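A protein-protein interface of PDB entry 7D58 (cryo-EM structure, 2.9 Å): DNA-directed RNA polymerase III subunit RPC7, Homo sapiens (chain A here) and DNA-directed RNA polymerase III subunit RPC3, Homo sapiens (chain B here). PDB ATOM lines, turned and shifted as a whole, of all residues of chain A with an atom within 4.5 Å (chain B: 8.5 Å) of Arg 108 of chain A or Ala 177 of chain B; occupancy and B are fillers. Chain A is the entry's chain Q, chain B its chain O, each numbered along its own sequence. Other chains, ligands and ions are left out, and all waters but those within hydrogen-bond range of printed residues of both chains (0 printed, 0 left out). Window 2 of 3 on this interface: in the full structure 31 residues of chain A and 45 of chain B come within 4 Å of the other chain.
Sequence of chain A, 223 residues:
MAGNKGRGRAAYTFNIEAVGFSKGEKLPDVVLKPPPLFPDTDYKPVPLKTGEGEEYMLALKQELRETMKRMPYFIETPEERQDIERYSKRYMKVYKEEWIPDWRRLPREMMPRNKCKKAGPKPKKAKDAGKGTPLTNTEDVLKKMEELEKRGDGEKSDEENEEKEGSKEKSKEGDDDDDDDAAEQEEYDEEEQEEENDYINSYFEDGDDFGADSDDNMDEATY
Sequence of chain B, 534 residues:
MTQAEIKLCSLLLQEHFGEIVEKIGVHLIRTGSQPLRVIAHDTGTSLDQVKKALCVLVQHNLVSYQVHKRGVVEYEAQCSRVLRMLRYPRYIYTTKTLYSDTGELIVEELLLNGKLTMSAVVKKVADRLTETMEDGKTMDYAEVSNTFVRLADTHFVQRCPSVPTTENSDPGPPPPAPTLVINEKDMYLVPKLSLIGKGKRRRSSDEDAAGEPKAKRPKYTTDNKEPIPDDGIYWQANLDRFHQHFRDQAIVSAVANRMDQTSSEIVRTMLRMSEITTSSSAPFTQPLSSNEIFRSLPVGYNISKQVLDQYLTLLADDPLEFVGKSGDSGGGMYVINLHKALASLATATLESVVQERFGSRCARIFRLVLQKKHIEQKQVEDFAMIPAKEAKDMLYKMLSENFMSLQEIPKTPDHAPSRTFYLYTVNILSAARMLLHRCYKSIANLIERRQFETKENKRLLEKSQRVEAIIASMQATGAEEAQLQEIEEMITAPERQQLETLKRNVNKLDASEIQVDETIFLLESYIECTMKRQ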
ATOM      1  N   LEU A 106      -8.076  -3.686   0.145  1.00  0.00           N
ATOM      2  CA  LEU A 106      -8.415  -3.044  -1.116  1.00  0.00           C
ATOM      3  C   LEU A 106      -8.820  -1.613  -0.807  1.00  0.00           C
ATOM      4  O   LEU A 106      -9.286  -1.319   0.302  1.00  0.00           O
ATOM      5  CB  LEU A 106      -9.549  -3.798  -1.825  1.00  0.00           C
ATOM      6  CG  LEU A 106      -9.941  -3.517  -3.277  1.00  0.00           C
ATOM      7  CD1 LEU A 106      -8.822  -3.931  -4.224  1.00  0.00           C
ATOM      8  CD2 LEU A 106     -11.233  -4.236  -3.624  1.00  0.00           C
ATOM      9  N   PRO A 107      -8.626  -0.691  -1.750  1.00  0.00           N
ATOM     10  CA  PRO A 107      -9.083   0.689  -1.538  1.00  0.00           C
ATOM     11  C   PRO A 107     -10.544   0.752  -1.116  1.00  0.00           C
ATOM     12  O   PRO A 107     -11.441   0.303  -1.834  1.00  0.00           O
ATOM     13  CB  PRO A 107      -8.857   1.342  -2.904  1.00  0.00           C
ATOM     14  CG  PRO A 107      -7.680   0.619  -3.455  1.00  0.00           C
ATOM     15  CD  PRO A 107      -7.761  -0.801  -2.940  1.00  0.00           C
ATOM     16  N   ARG A 108     -10.776   1.323   0.070  1.00  0.00           N
ATOM     17  CA  ARG A 108     -12.120   1.398   0.633  1.00  0.00           C
ATOM     18  C   ARG A 108     -13.024   2.333  -0.158  1.00  0.00           C
ATOM     19  O   ARG A 108     -14.252   2.206  -0.088  1.00  0.00           O
ATOM     20  CB  ARG A 108     -12.044   1.850   2.095  1.00  0.00           C
ATOM     21  CG  ARG A 108     -13.317   1.627   2.900  1.00  0.00           C
ATOM     22  CD  ARG A 108     -13.241   2.327   4.250  1.00  0.00           C
ATOM     23  NE  ARG A 108     -13.046   1.382   5.347  1.00  0.00           N
ATOM     24  CZ  ARG A 108     -13.044   1.717   6.633  1.00  0.00           C
ATOM     25  NH1 ARG A 108     -13.227   2.981   6.993  1.00  0.00           N
ATOM     26  NH2 ARG A 108     -12.859   0.789   7.561  1.00  0.00           N
ATOM     27  N   GLU A 109     -12.445   3.274  -0.906  1.00  0.00           N
ATOM     28  CA  GLU A 109     -13.248   4.174  -1.726  1.00  0.00           C
ATOM     29  C   GLU A 109     -13.970   3.407  -2.827  1.00  0.00           C
ATOM     30  O   GLU A 109     -15.161   3.622  -3.078  1.00  0.00           O
ATOM     31  CB  GLU A 109     -12.360   5.271  -2.317  1.00  0.00           C
ATOM     32  CG  GLU A 109     -13.125   6.462  -2.878  1.00  0.00           C
ATOM     33  CD  GLU A 109     -13.502   6.281  -4.335  1.00  0.00           C
ATOM     34  OE1 GLU A 109     -12.782   5.553  -5.052  1.00  0.00           O
ATOM     35  OE2 GLU A 109     -14.518   6.867  -4.765  1.00  0.00           O
ATOM     36  N   MET A 110     -13.260   2.501  -3.498  1.00  0.00           N
ATOM     37  CA  MET A 110     -13.854   1.708  -4.568  1.00  0.00           C
ATOM     38  C   MET A 110     -14.717   0.592  -3.994  1.00  0.00           C
ATOM     39  O   MET A 110     -14.199  -0.380  -3.436  1.00  0.00           O
ATOM     40  CB  MET A 110     -12.762   1.138  -5.478  1.00  0.00           C
ATOM     41  CG  MET A 110     -13.283   0.439  -6.728  1.00  0.00           C
ATOM     42  SD  MET A 110     -13.615  -1.317  -6.493  1.00  0.00           S
ATOM     43  CE  MET A 110     -11.946  -1.964  -6.433  1.00  0.00           C
ATOM     44  N   TYR B  65      -1.538   2.505  -5.660  1.00  0.00           N
ATOM     45  CA  TYR B  65      -2.426   3.621  -5.373  1.00  0.00           C
ATOM     46  C   TYR B  65      -1.946   4.317  -4.111  1.00  0.00           C
ATOM     47  O   TYR B  65      -1.374   3.686  -3.218  1.00  0.00           O
ATOM     48  CB  TYR B  65      -3.881   3.160  -5.214  1.00  0.00           C
ATOM     49  CG  TYR B  65      -4.117   2.241  -4.036  1.00  0.00           C
ATOM     50  CD1 TYR B  65      -4.601   2.734  -2.830  1.00  0.00           C
ATOM     51  CD2 TYR B  65      -3.859   0.879  -4.130  1.00  0.00           C
ATOM     52  CE1 TYR B  65      -4.819   1.898  -1.752  1.00  0.00           C
ATOM     53  CE2 TYR B  65      -4.074   0.036  -3.057  1.00  0.00           C
ATOM     54  CZ  TYR B  65      -4.553   0.551  -1.871  1.00  0.00           C
ATOM     55  OH  TYR B  65      -4.770  -0.283  -0.798  1.00  0.00           O
ATOM     56  N   VAL B  67      -2.705   7.938  -1.315  1.00  0.00           N
ATOM     57  CA  VAL B  67      -3.630   8.927  -0.774  1.00  0.00           C
ATOM     58  C   VAL B  67      -3.067  10.310  -1.065  1.00  0.00           C
ATOM     59  O   VAL B  67      -1.894  10.584  -0.783  1.00  0.00           O
ATOM     60  CB  VAL B  67      -3.844   8.728   0.736  1.00  0.00           C
ATOM     61  CG1 VAL B  67      -4.754   9.814   1.291  1.00  0.00           C
ATOM     62  CG2 VAL B  67      -4.406   7.344   1.019  1.00  0.00           C
ATOM     63  N   GLY B  71      -8.547  13.529   0.300  1.00  0.00           N
ATOM     64  CA  GLY B  71      -8.620  12.122   0.630  1.00  0.00           C
ATOM     65  C   GLY B  71      -8.530  11.259  -0.607  1.00  0.00           C
ATOM     66  O   GLY B  71      -8.905  10.083  -0.574  1.00  0.00           O
ATOM     67  N   VAL B  73      -7.710   9.144  -4.095  1.00  0.00           N
ATOM     68  CA  VAL B  73      -6.924   7.949  -4.376  1.00  0.00           C
ATOM     69  C   VAL B  73      -6.362   8.092  -5.787  1.00  0.00           C
ATOM     70  O   VAL B  73      -7.103   8.098  -6.775  1.00  0.00           O
ATOM     71  CB  VAL B  73      -7.752   6.670  -4.206  1.00  0.00           C
ATOM     72  CG1 VAL B  73      -7.955   6.369  -2.731  1.00  0.00           C
ATOM     73  CG2 VAL B  73      -9.106   6.807  -4.889  1.00  0.00           C
ATOM     74  N   TYR B  75      -4.099   6.454  -8.676  1.00  0.00           N
ATOM     75  CA  TYR B  75      -3.574   5.185  -9.150  1.00  0.00           C
ATOM     76  C   TYR B  75      -2.426   5.416 -10.127  1.00  0.00           C
ATOM     77  O   TYR B  75      -2.373   6.423 -10.837  1.00  0.00           O
ATOM     78  CB  TYR B  75      -4.678   4.362  -9.817  1.00  0.00           C
ATOM     79  CG  TYR B  75      -5.941   4.261  -8.994  1.00  0.00           C
ATOM     80  CD1 TYR B  75      -6.070   3.297  -8.003  1.00  0.00           C
ATOM     81  CD2 TYR B  75      -7.005   5.128  -9.208  1.00  0.00           C
ATOM     82  CE1 TYR B  75      -7.221   3.202  -7.247  1.00  0.00           C
ATOM     83  CE2 TYR B  75      -8.160   5.039  -8.456  1.00  0.00           C
ATOM     84  CZ  TYR B  75      -8.262   4.074  -7.478  1.00  0.00           C
ATOM     85  OH  TYR B  75      -9.410   3.979  -6.725  1.00  0.00           O
ATOM     86  N   ALA B 177     -11.151   7.114   7.660  1.00  0.00           N
ATOM     87  CA  ALA B 177     -10.168   7.117   6.584  1.00  0.00           C
ATOM     88  C   ALA B 177     -10.808   6.719   5.258  1.00  0.00           C
ATOM     89  O   ALA B 177     -11.626   5.801   5.211  1.00  0.00           O
ATOM     90  CB  ALA B 177      -9.014   6.182   6.917  1.00  0.00           C
ATOM     91  N   PRO B 178     -10.437   7.413   4.178  1.00  0.00           N
ATOM     92  CA  PRO B 178     -10.978   7.064   2.857  1.00  0.00           C
ATOM     93  C   PRO B 178     -10.511   5.693   2.399  1.00  0.00           C
ATOM     94  O   PRO B 178     -11.239   4.974   1.709  1.00  0.00           O
ATOM     95  CB  PRO B 178     -10.441   8.179   1.950  1.00  0.00           C
ATOM     96  CG  PRO B 178      -9.216   8.673   2.646  1.00  0.00           C
ATOM     97  CD  PRO B 178      -9.498   8.547   4.115  1.00  0.00           C
ATOM     98  N   THR B 179      -9.291   5.327   2.786  1.00  0.00           N
ATOM     99  CA  THR B 179      -8.749   4.007   2.503  1.00  0.00           C
ATOM    100  C   THR B 179      -7.642   3.714   3.503  1.00  0.00           C
ATOM    101  O   THR B 179      -7.229   4.581   4.278  1.00  0.00           O
ATOM    102  CB  THR B 179      -8.224   3.902   1.066  1.00  0.00           C
ATOM    103  OG1 THR B 179      -7.833   2.551   0.797  1.00  0.00           O
ATOM    104  CG2 THR B 179      -7.028   4.818   0.869  1.00  0.00           C
ATOM    105  N   LEU B 180      -7.160   2.476   3.479  1.00  0.00           N
ATOM    106  CA  LEU B 180      -6.109   2.044   4.388  1.00  0.00           C
ATOM    107  C   LEU B 180      -4.749   2.158   3.711  1.00  0.00           C
ATOM    108  O   LEU B 180      -4.597   1.834   2.531  1.00  0.00           O
ATOM    109  CB  LEU B 180      -6.349   0.607   4.859  1.00  0.00           C
ATOM    110  CG  LEU B 180      -6.109  -0.570   3.905  1.00  0.00           C
ATOM    111  CD1 LEU B 180      -6.002  -1.868   4.689  1.00  0.00           C
ATOM    112  CD2 LEU B 180      -7.206  -0.676   2.856  1.00  0.00           C
ATOM    113  N   VAL B 181      -3.766   2.641   4.466  1.00  0.00           N
ATOM    114  CA  VAL B 181      -2.398   2.752   3.969  1.00  0.00           C
ATOM    115  C   VAL B 181      -1.694   1.414   4.189  1.00  0.00           C
ATOM    116  O   VAL B 181      -1.472   0.986   5.324  1.00  0.00           O
ATOM    117  CB  VAL B 181      -1.646   3.915   4.632  1.00  0.00           C
ATOM    118  CG1 VAL B 181      -1.678   3.819   6.158  1.00  0.00           C
ATOM    119  CG2 VAL B 181      -0.210   3.967   4.129  1.00  0.00           C
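N of Glu 109 of chain A lies within hydrogen-bond range of O of Pro 178 of chain B.
OG1 of Thr 179 of chain B sits at hydrogen-bond distance from N of Arg 108 of chain A.
Among the printed residues, merely in contact across the chains: Pro 107 of chain A with Thr 179 of chain B (3.2 Å), Arg 108 of chain A with Pro 178 of chain B (3.2 Å), Leu 106 of chain A with Leu 180 of chain B (3.4 Å), Pro 107 of chain A with Tyr 65 of chain B (3.5 Å), Arg 108 of chain A with Ala 177 of chain B (3.7 Å) and Glu 109 of chain A with Val 73 of chain B (3.9 Å).
Of the printed residues of chain B, Pro 107 of chain A touches Tyr 65 (3.5 Å) and Thr 179 (3.2 Å).
Arg 108 of chain A touches just these residues of chain B: Ala 177 (3.7 Å), Pro 178 (3.2 Å) and Thr 179 (3.3 Å).
Printed residues of chain B within 4 Å of Glu 109 of chain A: Val 73 and Pro 178.
Val 67 of chain B touches none of the printed residues of chain A.
Of the printed residues of chain A, Leu 180 of chain B touches Leu 106 (3.4 Å).
Of the 10 printed residues of chain B, 6 touch a printed residue of chain A.
Hydrophobic or aromatic side chains of chain B within 4 Å of the printed part of chain A: Tyr 65, Val 73 and Leu 180.
Among the printed residues, 8 pairs touch across the chains.
Among the printed residues, no Asp or Glu carboxylate lies within 4 Å of a Lys or Arg side-chain nitrogen of the other chain.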
